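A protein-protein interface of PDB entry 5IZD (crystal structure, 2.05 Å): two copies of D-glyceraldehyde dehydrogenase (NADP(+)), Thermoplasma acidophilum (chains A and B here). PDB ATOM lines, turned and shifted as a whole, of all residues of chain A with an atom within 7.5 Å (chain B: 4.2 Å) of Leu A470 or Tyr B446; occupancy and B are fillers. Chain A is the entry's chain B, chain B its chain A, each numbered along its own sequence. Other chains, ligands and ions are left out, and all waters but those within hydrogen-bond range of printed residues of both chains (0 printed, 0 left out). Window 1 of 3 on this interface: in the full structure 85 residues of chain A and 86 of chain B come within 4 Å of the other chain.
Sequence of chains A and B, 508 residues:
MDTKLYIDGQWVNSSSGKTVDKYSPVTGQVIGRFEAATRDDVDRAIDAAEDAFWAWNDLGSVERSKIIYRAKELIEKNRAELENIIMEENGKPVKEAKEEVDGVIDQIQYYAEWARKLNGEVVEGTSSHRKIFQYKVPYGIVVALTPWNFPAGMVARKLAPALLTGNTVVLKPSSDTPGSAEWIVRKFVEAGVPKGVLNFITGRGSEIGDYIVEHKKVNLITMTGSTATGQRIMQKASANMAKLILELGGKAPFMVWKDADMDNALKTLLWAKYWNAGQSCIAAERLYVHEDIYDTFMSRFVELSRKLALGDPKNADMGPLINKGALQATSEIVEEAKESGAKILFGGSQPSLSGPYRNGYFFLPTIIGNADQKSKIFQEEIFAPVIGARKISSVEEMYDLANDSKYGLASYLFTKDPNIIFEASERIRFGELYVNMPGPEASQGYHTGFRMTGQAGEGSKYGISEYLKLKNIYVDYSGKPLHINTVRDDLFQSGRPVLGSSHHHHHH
Of the 12 printed residues of chain B, 4 touch a printed residue of chain A. Printed residues of chain B that touch a printed residue of chain A: Gly B445, Tyr B446, Thr B448 and Tyr B462. Along chain B the printed residues that touch a printed residue of chain A span positions 445 to 462. Among the printed residues, 11 pairs touch across the chains.
Asn A119 touches none of the printed residues of chain B. Val A123 touches none of the printed residues of chain B. Of the printed residues of chain B, Leu A470 touches Tyr B446 (3.8 Å), Thr B448 (3.2 Å) and Tyr B462 (3.4 Å). Printed residues of chain B within 4 Å of Tyr A474: Gly B445 (3.8 Å). Printed residues of chain A within 4 Å of Tyr B446: Gln A134, Leu A470 and Asn A472. Printed residues of chain A within 4 Å of Tyr B462: Glu A121, Lys A136 and Leu A470. The nearest printed residue of chain B that does not touch Leu A470 is Ser B460 (5.0 Å). The nearest printed residue of chain A that does not touch Tyr B446 is Lys A469 (5.1 Å). The nearest printed residue of chain B that does not touch Tyr A474 is Tyr B446 (5.1 Å).
The side-chain hydroxyl (OH) of Tyr B462 is in hydrogen-bond range of the side-chain carboxylate (OE2) of Glu A121, at 2.6 Å. ND2 of Asn A472 is in hydrogen-bond range of O of Tyr B446 (2.7 Å). The side-chain amide nitrogen (NE2) of Gln A134 sits close to the backbone NH (N) of Tyr B446 (3.4 Å). The side-chain hydroxyl (OH) of Tyr B462 is in hydrogen-bond range of the side-chain amino group (NZ) of Lys A136 (3.4 Å). The side-chain hydroxyl (OG1) of Thr B448 is in hydrogen-bond range of the side-chain amino group (NZ) of Lys A469, 3.1 Å away.
The side-chain hydroxyl of Tyr B446 sits at hydrogen-bond distance from the backbone NH of Gly B457 (3.1 Å). OG of Ser B460 is in hydrogen-bond range of N of Tyr B462 (3.0 Å). O of Glu A121 is in hydrogen-bond range of N of Gln A134 (2.8 Å). The side-chain carboxylate (OE2) of Glu B466 is in hydrogen-bond range of the side-chain hydroxyl (OH) of Tyr B446 (2.8 Å). N of Ser B460 lies within hydrogen-bond range of O of Gly B445. The backbone NH (N) of Lys A469 is in hydrogen-bond range of the backbone carbonyl oxygen (O) of Val A137, 2.8 Å away.
No position is printed for both chains.
Among the printed residues, merely in contact across the chains: Leu A470 with Thr B448 (3.2 Å), Leu A470 with Tyr B462 (3.4 Å), Gln A134 with Gly B445 (3.6 Å), Leu A470 with Tyr B446 (3.8 Å), Tyr A474 with Gly B445 (3.8 Å) and Asn A472 with Gly B445 (3.8 Å).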
ATOM      1  N   ASN A 119     -13.005  10.318 -25.645  1.00  0.00           N
ATOM      2  CA  ASN A 119     -11.873  11.117 -26.130  1.00  0.00           C
ATOM      3  C   ASN A 119     -10.844  11.526 -25.043  1.00  0.00           C
ATOM      4  O   ASN A 119     -11.165  11.620 -23.906  1.00  0.00           O
ATOM      5  CB  ASN A 119     -12.468  12.388 -26.754  1.00  0.00           C
ATOM      6  CG  ASN A 119     -13.224  13.302 -25.716  1.00  0.00           C
ATOM      7  OD1 ASN A 119     -14.481  13.251 -25.584  1.00  0.00           O
ATOM      8  ND2 ASN A 119     -12.467  14.187 -25.024  1.00  0.00           N
ATOM      9  N   GLY A 120      -9.611  11.739 -25.460  1.00  0.00           N
ATOM     10  CA  GLY A 120      -8.594  12.361 -24.651  1.00  0.00           C
ATOM     11  C   GLY A 120      -8.675  13.835 -24.987  1.00  0.00           C
ATOM     12  O   GLY A 120      -9.642  14.292 -25.634  1.00  0.00           O
ATOM     13  N   GLU A 121      -7.638  14.569 -24.617  1.00  0.00           N
ATOM     14  CA  GLU A 121      -7.628  16.045 -24.713  1.00  0.00           C
ATOM     15  C   GLU A 121      -6.328  16.524 -25.252  1.00  0.00           C
ATOM     16  O   GLU A 121      -5.346  15.821 -25.166  1.00  0.00           O
ATOM     17  CB  GLU A 121      -7.943  16.693 -23.348  1.00  0.00           C
ATOM     18  CG  GLU A 121      -9.246  16.080 -22.818  1.00  0.00           C
ATOM     19  CD  GLU A 121     -10.098  16.919 -21.895  1.00  0.00           C
ATOM     20  OE1 GLU A 121      -9.701  18.023 -21.527  1.00  0.00           O
ATOM     21  OE2 GLU A 121     -11.204  16.435 -21.520  1.00  0.00           O
ATOM     22  N   VAL A 123      -4.230  20.197 -24.784  1.00  0.00           N
ATOM     23  CA  VAL A 123      -4.210  21.514 -24.137  1.00  0.00           C
ATOM     24  C   VAL A 123      -2.934  22.284 -24.503  1.00  0.00           C
ATOM     25  O   VAL A 123      -1.927  21.737 -24.975  1.00  0.00           O
ATOM     26  CB  VAL A 123      -4.374  21.463 -22.597  1.00  0.00           C
ATOM     27  CG1 VAL A 123      -5.729  20.959 -22.162  1.00  0.00           C
ATOM     28  CG2 VAL A 123      -3.325  20.619 -21.960  1.00  0.00           C
ATOM     29  N   ILE A 132       0.370  19.737 -24.824  1.00  0.00           N
ATOM     30  CA  ILE A 132       0.190  18.614 -23.918  1.00  0.00           C
ATOM     31  C   ILE A 132      -0.942  17.728 -24.470  1.00  0.00           C
ATOM     32  O   ILE A 132      -2.095  18.159 -24.571  1.00  0.00           O
ATOM     33  CB  ILE A 132      -0.108  19.058 -22.498  1.00  0.00           C
ATOM     34  CG1 ILE A 132       0.990  20.063 -22.034  1.00  0.00           C
ATOM     35  CG2 ILE A 132      -0.181  17.854 -21.544  1.00  0.00           C
ATOM     36  CD1 ILE A 132       0.721  20.769 -20.724  1.00  0.00           C
ATOM     37  N   PHE A 133      -0.616  16.502 -24.830  1.00  0.00           N
ATOM     38  CA  PHE A 133      -1.618  15.531 -25.310  1.00  0.00           C
ATOM     39  C   PHE A 133      -1.988  14.680 -24.121  1.00  0.00           C
ATOM     40  O   PHE A 133      -1.112  14.263 -23.336  1.00  0.00           O
ATOM     41  CB  PHE A 133      -1.004  14.697 -26.405  1.00  0.00           C
ATOM     42  CG  PHE A 133      -0.640  15.506 -27.605  1.00  0.00           C
ATOM     43  CD1 PHE A 133      -1.626  15.971 -28.453  1.00  0.00           C
ATOM     44  CD2 PHE A 133       0.664  15.922 -27.820  1.00  0.00           C
ATOM     45  CE1 PHE A 133      -1.314  16.754 -29.548  1.00  0.00           C
ATOM     46  CE2 PHE A 133       1.001  16.706 -28.905  1.00  0.00           C
ATOM     47  CZ  PHE A 133       0.009  17.131 -29.776  1.00  0.00           C
ATOM     48  N   GLN A 134      -3.279  14.501 -23.897  1.00  0.00           N
ATOM     49  CA  GLN A 134      -3.760  13.674 -22.806  1.00  0.00           C
ATOM     50  C   GLN A 134      -4.532  12.496 -23.381  1.00  0.00           C
ATOM     51  O   GLN A 134      -5.648  12.681 -23.853  1.00  0.00           O
ATOM     52  CB  GLN A 134      -4.616  14.482 -21.875  1.00  0.00           C
ATOM     53  CG  GLN A 134      -3.782  15.621 -21.284  1.00  0.00           C
ATOM     54  CD  GLN A 134      -4.548  16.529 -20.351  1.00  0.00           C
ATOM     55  OE1 GLN A 134      -5.717  16.865 -20.596  1.00  0.00           O
ATOM     56  NE2 GLN A 134      -3.878  16.951 -19.249  1.00  0.00           N
ATOM     57  N   TYR A 135      -3.912  11.323 -23.369  1.00  0.00           N
ATOM     58  CA  TYR A 135      -4.524  10.134 -23.848  1.00  0.00           C
ATOM     59  C   TYR A 135      -5.271   9.466 -22.711  1.00  0.00           C
ATOM     60  O   TYR A 135      -4.829   9.484 -21.534  1.00  0.00           O
ATOM     61  CB  TYR A 135      -3.430   9.207 -24.367  1.00  0.00           C
ATOM     62  CG  TYR A 135      -2.826   9.490 -25.738  1.00  0.00           C
ATOM     63  CD1 TYR A 135      -2.772  10.759 -26.280  1.00  0.00           C
ATOM     64  CD2 TYR A 135      -2.270   8.477 -26.465  1.00  0.00           C
ATOM     65  CE1 TYR A 135      -2.212  10.984 -27.508  1.00  0.00           C
ATOM     66  CE2 TYR A 135      -1.678   8.704 -27.703  1.00  0.00           C
ATOM     67  CZ  TYR A 135      -1.670   9.973 -28.227  1.00  0.00           C
ATOM     68  OH  TYR A 135      -1.087  10.233 -29.433  1.00  0.00           O
ATOM     69  N   LYS A 136      -6.393   8.856 -23.014  1.00  0.00           N
ATOM     70  CA  LYS A 136      -7.052   7.931 -22.097  1.00  0.00           C
ATOM     71  C   LYS A 136      -6.775   6.480 -22.543  1.00  0.00           C
ATOM     72  O   LYS A 136      -7.107   6.100 -23.690  1.00  0.00           O
ATOM     73  CB  LYS A 136      -8.556   8.215 -22.077  1.00  0.00           C
ATOM     74  CG  LYS A 136      -8.915   9.397 -21.219  1.00  0.00           C
ATOM     75  CD  LYS A 136     -10.420   9.513 -21.168  1.00  0.00           C
ATOM     76  CE  LYS A 136     -10.704  10.894 -20.650  1.00  0.00           C
ATOM     77  NZ  LYS A 136     -12.139  11.057 -20.303  1.00  0.00           N
ATOM     78  N   VAL A 137      -6.159   5.676 -21.692  1.00  0.00           N
ATOM     79  CA  VAL A 137      -5.787   4.309 -21.994  1.00  0.00           C
ATOM     80  C   VAL A 137      -6.250   3.350 -20.934  1.00  0.00           C
ATOM     81  O   VAL A 137      -6.663   3.779 -19.914  1.00  0.00           O
ATOM     82  CB  VAL A 137      -4.274   4.191 -22.171  1.00  0.00           C
ATOM     83  CG1 VAL A 137      -3.820   5.111 -23.260  1.00  0.00           C
ATOM     84  CG2 VAL A 137      -3.544   4.447 -20.868  1.00  0.00           C
ATOM     85  N   PRO A 138      -6.208   2.047 -21.180  1.00  0.00           N
ATOM     86  CA  PRO A 138      -6.679   1.161 -20.135  1.00  0.00           C
ATOM     87  C   PRO A 138      -5.722   1.029 -18.961  1.00  0.00           C
ATOM     88  O   PRO A 138      -4.562   1.244 -19.077  1.00  0.00           O
ATOM     89  CB  PRO A 138      -6.828  -0.186 -20.834  1.00  0.00           C
ATOM     90  CG  PRO A 138      -6.122  -0.077 -22.099  1.00  0.00           C
ATOM     91  CD  PRO A 138      -5.993   1.348 -22.450  1.00  0.00           C
ATOM     92  N   TYR A 139      -6.258   0.691 -17.824  1.00  0.00           N
ATOM     93  CA  TYR A 139      -5.405   0.416 -16.648  1.00  0.00           C
ATOM     94  C   TYR A 139      -4.648  -0.866 -16.841  1.00  0.00           C
ATOM     95  O   TYR A 139      -3.588  -0.990 -16.345  1.00  0.00           O
ATOM     96  CB  TYR A 139      -6.241   0.292 -15.380  1.00  0.00           C
ATOM     97  CG  TYR A 139      -6.598   1.579 -14.782  1.00  0.00           C
ATOM     98  CD1 TYR A 139      -7.715   2.277 -15.210  1.00  0.00           C
ATOM     99  CD2 TYR A 139      -5.818   2.118 -13.741  1.00  0.00           C
ATOM    100  CE1 TYR A 139      -8.057   3.498 -14.641  1.00  0.00           C
ATOM    101  CE2 TYR A 139      -6.158   3.342 -13.168  1.00  0.00           C
ATOM    102  CZ  TYR A 139      -7.282   4.009 -13.628  1.00  0.00           C
ATOM    103  OH  TYR A 139      -7.651   5.216 -13.074  1.00  0.00           O
ATOM    104  N   SER A 465     -15.485   5.804 -17.680  1.00  0.00           N
ATOM    105  CA  SER A 465     -14.161   6.445 -17.617  1.00  0.00           C
ATOM    106  C   SER A 465     -13.343   6.079 -16.424  1.00  0.00           C
ATOM    107  O   SER A 465     -12.162   6.283 -16.465  1.00  0.00           O
ATOM    108  CB  SER A 465     -14.280   7.960 -17.630  1.00  0.00           C
ATOM    109  OG  SER A 465     -14.895   8.358 -18.823  1.00  0.00           O
ATOM    110  N   LEU A 468     -10.418   3.870 -17.454  1.00  0.00           N
ATOM    111  CA  LEU A 468      -9.435   4.508 -18.304  1.00  0.00           C
ATOM    112  C   LEU A 468      -8.511   5.402 -17.436  1.00  0.00           C
ATOM    113  O   LEU A 468      -8.955   6.140 -16.593  1.00  0.00           O
ATOM    114  CB  LEU A 468     -10.137   5.375 -19.380  1.00  0.00           C
ATOM    115  CG  LEU A 468     -10.818   4.575 -20.492  1.00  0.00           C
ATOM    116  CD1 LEU A 468     -11.793   5.403 -21.303  1.00  0.00           C
ATOM    117  CD2 LEU A 468      -9.750   4.031 -21.424  1.00  0.00           C
ATOM    118  N   LYS A 469      -7.224   5.274 -17.663  1.00  0.00           N
ATOM    119  CA  LYS A 469      -6.227   6.123 -17.064  1.00  0.00           C
ATOM    120  C   LYS A 469      -5.872   7.226 -18.044  1.00  0.00           C
ATOM    121  O   LYS A 469      -5.552   6.968 -19.216  1.00  0.00           O
ATOM    122  CB  LYS A 469      -4.982   5.285 -16.782  1.00  0.00           C
ATOM    123  CG  LYS A 469      -3.912   6.040 -16.004  1.00  0.00           C
ATOM    124  CD  LYS A 469      -4.313   6.104 -14.531  1.00  0.00           C
ATOM    125  CE  LYS A 469      -3.617   7.209 -13.806  1.00  0.00           C
ATOM    126  NZ  LYS A 469      -3.855   7.020 -12.365  1.00  0.00           N
ATOM    127  N   LEU A 470      -5.831   8.432 -17.543  1.00  0.00           N
ATOM    128  CA  LEU A 470      -5.405   9.528 -18.333  1.00  0.00           C
ATOM    129  C   LEU A 470      -3.868   9.710 -18.188  1.00  0.00           C
ATOM    130  O   LEU A 470      -3.364   9.765 -17.095  1.00  0.00           O
ATOM    131  CB  LEU A 470      -6.182  10.738 -17.883  1.00  0.00           C
ATOM    132  CG  LEU A 470      -6.271  12.052 -18.614  1.00  0.00           C
ATOM    133  CD1 LEU A 470      -6.941  12.003 -19.958  1.00  0.00           C
ATOM    134  CD2 LEU A 470      -6.935  13.091 -17.741  1.00  0.00           C
ATOM    135  N   LYS A 471      -3.138   9.750 -19.287  1.00  0.00           N
ATOM    136  CA  LYS A 471      -1.691  10.017 -19.330  1.00  0.00           C
ATOM    137  C   LYS A 471      -1.389  11.257 -20.201  1.00  0.00           C
ATOM    138  O   LYS A 471      -2.125  11.545 -21.143  1.00  0.00           O
ATOM    139  CB  LYS A 471      -0.903   8.769 -19.831  1.00  0.00           C
ATOM    140  CG  LYS A 471      -1.008   8.533 -21.355  1.00  0.00           C
ATOM    141  CD  LYS A 471      -0.709   7.102 -21.810  1.00  0.00           C
ATOM    142  CE  LYS A 471       0.721   6.616 -21.528  1.00  0.00           C
ATOM    143  NZ  LYS A 471       1.862   7.348 -22.157  1.00  0.00           N
ATOM    144  N   ASN A 472      -0.258  11.912 -19.948  1.00  0.00           N
ATOM    145  CA  ASN A 472       0.127  13.167 -20.609  1.00  0.00           C
ATOM    146  C   ASN A 472       1.423  12.976 -21.407  1.00  0.00           C
ATOM    147  O   ASN A 472       2.401  12.335 -20.926  1.00  0.00           O
ATOM    148  CB  ASN A 472       0.374  14.322 -19.622  1.00  0.00           C
ATOM    149  CG  ASN A 472      -0.705  14.475 -18.553  1.00  0.00           C
ATOM    150  OD1 ASN A 472      -1.535  15.370 -18.596  1.00  0.00           O
ATOM    151  ND2 ASN A 472      -0.668  13.599 -17.571  1.00  0.00           N
ATOM    152  N   TYR A 474       3.994  15.638 -23.212  1.00  0.00           N
ATOM    153  CA  TYR A 474       4.408  17.023 -23.312  1.00  0.00           C
ATOM    154  C   TYR A 474       5.371  17.005 -24.438  1.00  0.00           C
ATOM    155  O   TYR A 474       6.481  16.431 -24.274  1.00  0.00           O
ATOM    156  CB  TYR A 474       5.177  17.503 -22.028  1.00  0.00           C
ATOM    157  CG  TYR A 474       4.339  17.811 -20.808  1.00  0.00           C
ATOM    158  CD1 TYR A 474       3.671  16.812 -20.136  1.00  0.00           C
ATOM    159  CD2 TYR A 474       4.206  19.099 -20.331  1.00  0.00           C
ATOM    160  CE1 TYR A 474       2.897  17.064 -19.012  1.00  0.00           C
ATOM    161  CE2 TYR A 474       3.441  19.390 -19.196  1.00  0.00           C
ATOM    162  CZ  TYR A 474       2.790  18.360 -18.528  1.00  0.00           C
ATOM    163  OH  TYR A 474       2.014  18.622 -17.410  1.00  0.00           O
ATOM    164  N   GLY B 445      -1.951  20.303 -17.020  1.00  0.00           N
ATOM    165  CA  GLY B 445      -1.731  18.850 -17.050  1.00  0.00           C
ATOM    166  C   GLY B 445      -2.354  18.048 -15.922  1.00  0.00           C
ATOM    167  O   GLY B 445      -2.631  18.579 -14.892  1.00  0.00           O
ATOM    168  N   TYR B 446      -2.590  16.766 -16.106  1.00  0.00           N
ATOM    169  CA  TYR B 446      -3.156  15.950 -15.057  1.00  0.00           C
ATOM    170  C   TYR B 446      -2.014  15.110 -14.531  1.00  0.00           C
ATOM    171  O   TYR B 446      -1.669  14.128 -15.105  1.00  0.00           O
ATOM    172  CB  TYR B 446      -4.303  15.093 -15.560  1.00  0.00           C
ATOM    173  CG  TYR B 446      -4.959  14.184 -14.562  1.00  0.00           C
ATOM    174  CD1 TYR B 446      -5.769  14.683 -13.574  1.00  0.00           C
ATOM    175  CD2 TYR B 446      -4.816  12.830 -14.635  1.00  0.00           C
ATOM    176  CE1 TYR B 446      -6.380  13.863 -12.692  1.00  0.00           C
ATOM    177  CE2 TYR B 446      -5.437  12.005 -13.751  1.00  0.00           C
ATOM    178  CZ  TYR B 446      -6.214  12.540 -12.782  1.00  0.00           C
ATOM    179  OH  TYR B 446      -6.817  11.747 -11.900  1.00  0.00           O
ATOM    180  N   HIS B 447      -1.432  15.538 -13.426  1.00  0.00           N
ATOM    181  CA  HIS B 447      -0.264  14.925 -12.826  1.00  0.00           C
ATOM    182  C   HIS B 447      -0.681  13.640 -12.126  1.00  0.00           C
ATOM    183  O   HIS B 447      -1.397  13.688 -11.135  1.00  0.00           O
ATOM    184  CB  HIS B 447       0.315  15.894 -11.778  1.00  0.00           C
ATOM    185  CG  HIS B 447       1.693  15.577 -11.302  1.00  0.00           C
ATOM    186  ND1 HIS B 447       2.764  15.498 -12.164  1.00  0.00           N
ATOM    187  CD2 HIS B 447       2.217  15.502 -10.044  1.00  0.00           C
ATOM    188  CE1 HIS B 447       3.881  15.330 -11.465  1.00  0.00           C
ATOM    189  NE2 HIS B 447       3.570  15.304 -10.180  1.00  0.00           N
ATOM    190  N   THR B 448      -0.193  12.507 -12.606  1.00  0.00           N
ATOM    191  CA  THR B 448      -0.687  11.218 -12.184  1.00  0.00           C
ATOM    192  C   THR B 448       0.294  10.161 -12.686  1.00  0.00           C
ATOM    193  O   THR B 448       1.274  10.456 -13.381  1.00  0.00           O
ATOM    194  CB  THR B 448      -2.131  11.006 -12.793  1.00  0.00           C
ATOM    195  OG1 THR B 448      -2.800   9.914 -12.160  1.00  0.00           O
ATOM    196  CG2 THR B 448      -2.056  10.753 -14.289  1.00  0.00           C
ATOM    197  N   ALA B 456      -5.597   8.693  -8.127  1.00  0.00           N
ATOM    198  CA  ALA B 456      -6.163   9.832  -8.772  1.00  0.00           C
ATOM    199  C   ALA B 456      -5.041  10.714  -9.344  1.00  0.00           C
ATOM    200  O   ALA B 456      -4.048  10.176  -9.812  1.00  0.00           O
ATOM    201  CB  ALA B 456      -7.093  10.556  -7.844  1.00  0.00           C
ATOM    202  N   GLY B 457      -5.175  12.038  -9.317  1.00  0.00           N
ATOM    203  CA  GLY B 457      -4.176  12.932  -9.879  1.00  0.00           C
ATOM    204  C   GLY B 457      -4.547  14.366  -9.536  1.00  0.00           C
ATOM    205  O   GLY B 457      -5.605  14.582  -8.933  1.00  0.00           O
ATOM    206  N   GLU B 458      -3.690  15.303  -9.947  1.00  0.00           N
ATOM    207  CA  GLU B 458      -3.815  16.740  -9.687  1.00  0.00           C
ATOM    208  C   GLU B 458      -3.490  17.615 -10.897  1.00  0.00           C
ATOM    209  O   GLU B 458      -2.583  17.332 -11.666  1.00  0.00           O
ATOM    210  CB  GLU B 458      -2.895  17.126  -8.543  1.00  0.00           C
ATOM    211  CG  GLU B 458      -3.226  16.410  -7.261  1.00  0.00           C
ATOM    212  CD  GLU B 458      -2.153  16.614  -6.165  1.00  0.00           C
ATOM    213  OE1 GLU B 458      -2.387  17.320  -5.117  1.00  0.00           O
ATOM    214  OE2 GLU B 458      -1.060  16.032  -6.403  1.00  0.00           O
ATOM    215  N   GLY B 459      -4.231  18.685 -11.053  1.00  0.00           N
ATOM    216  CA  GLY B 459      -4.106  19.523 -12.185  1.00  0.00           C
ATOM    217  C   GLY B 459      -5.074  19.173 -13.280  1.00  0.00           C
ATOM    218  O   GLY B 459      -5.561  18.047 -13.385  1.00  0.00           O
ATOM    219  N   SER B 460      -5.308  20.139 -14.148  1.00  0.00           N
ATOM    220  CA  SER B 460      -6.320  20.062 -15.201  1.00  0.00           C
ATOM    221  C   SER B 460      -7.739  20.093 -14.654  1.00  0.00           C
ATOM    222  O   SER B 460      -7.991  20.020 -13.467  1.00  0.00           O
ATOM    223  CB  SER B 460      -6.114  18.843 -16.150  1.00  0.00           C
ATOM    224  OG  SER B 460      -6.802  17.660 -15.712  1.00  0.00           O
ATOM    225  N   TYR B 462      -9.637  17.631 -14.786  1.00  0.00           N
ATOM    226  CA  TYR B 462      -9.828  16.385 -14.092  1.00  0.00           C
ATOM    227  C   TYR B 462      -9.281  16.438 -12.662  1.00  0.00           C
ATOM    228  O   TYR B 462      -9.814  15.797 -11.798  1.00  0.00           O
ATOM    229  CB  TYR B 462      -9.167  15.224 -14.857  1.00  0.00           C
ATOM    230  CG  TYR B 462      -9.834  14.986 -16.214  1.00  0.00           C
ATOM    231  CD1 TYR B 462     -11.015  14.270 -16.318  1.00  0.00           C
ATOM    232  CD2 TYR B 462      -9.277  15.483 -17.376  1.00  0.00           C
ATOM    233  CE1 TYR B 462     -11.675  14.103 -17.599  1.00  0.00           C
ATOM    234  CE2 TYR B 462      -9.896  15.297 -18.628  1.00  0.00           C
ATOM    235  CZ  TYR B 462     -11.091  14.618 -18.731  1.00  0.00           C
ATOM    236  OH  TYR B 462     -11.657  14.397 -20.013  1.00  0.00           O
ATOM    237  N   GLY B 463      -8.190  17.141 -12.450  1.00  0.00           N
ATOM    238  CA  GLY B 463      -7.573  17.252 -11.099  1.00  0.00           C
ATOM    239  C   GLY B 463      -8.442  18.013 -10.111  1.00  0.00           C
ATOM    240  O   GLY B 463      -8.727  17.533  -9.025  1.00  0.00           O
ATOM    241  N   GLU B 466     -11.444  16.143  -8.956  1.00  0.00           N
ATOM    242  CA  GLU B 466     -11.244  15.135  -7.919  1.00  0.00           C
ATOM    243  C   GLU B 466     -11.762  15.608  -6.579  1.00  0.00           C
ATOM    244  O   GLU B 466     -12.019  14.774  -5.701  1.00  0.00           O
ATOM    245  CB  GLU B 466      -9.765  14.700  -7.757  1.00  0.00           C
ATOM    246  CG  GLU B 466      -9.129  14.041  -8.992  1.00  0.00           C
ATOM    247  CD  GLU B 466      -9.668  12.648  -9.394  1.00  0.00           C
ATOM    248  OE1 GLU B 466     -10.660  12.122  -8.814  1.00  0.00           O
ATOM    249  OE2 GLU B 466      -9.064  12.066 -10.336  1.00  0.00           O
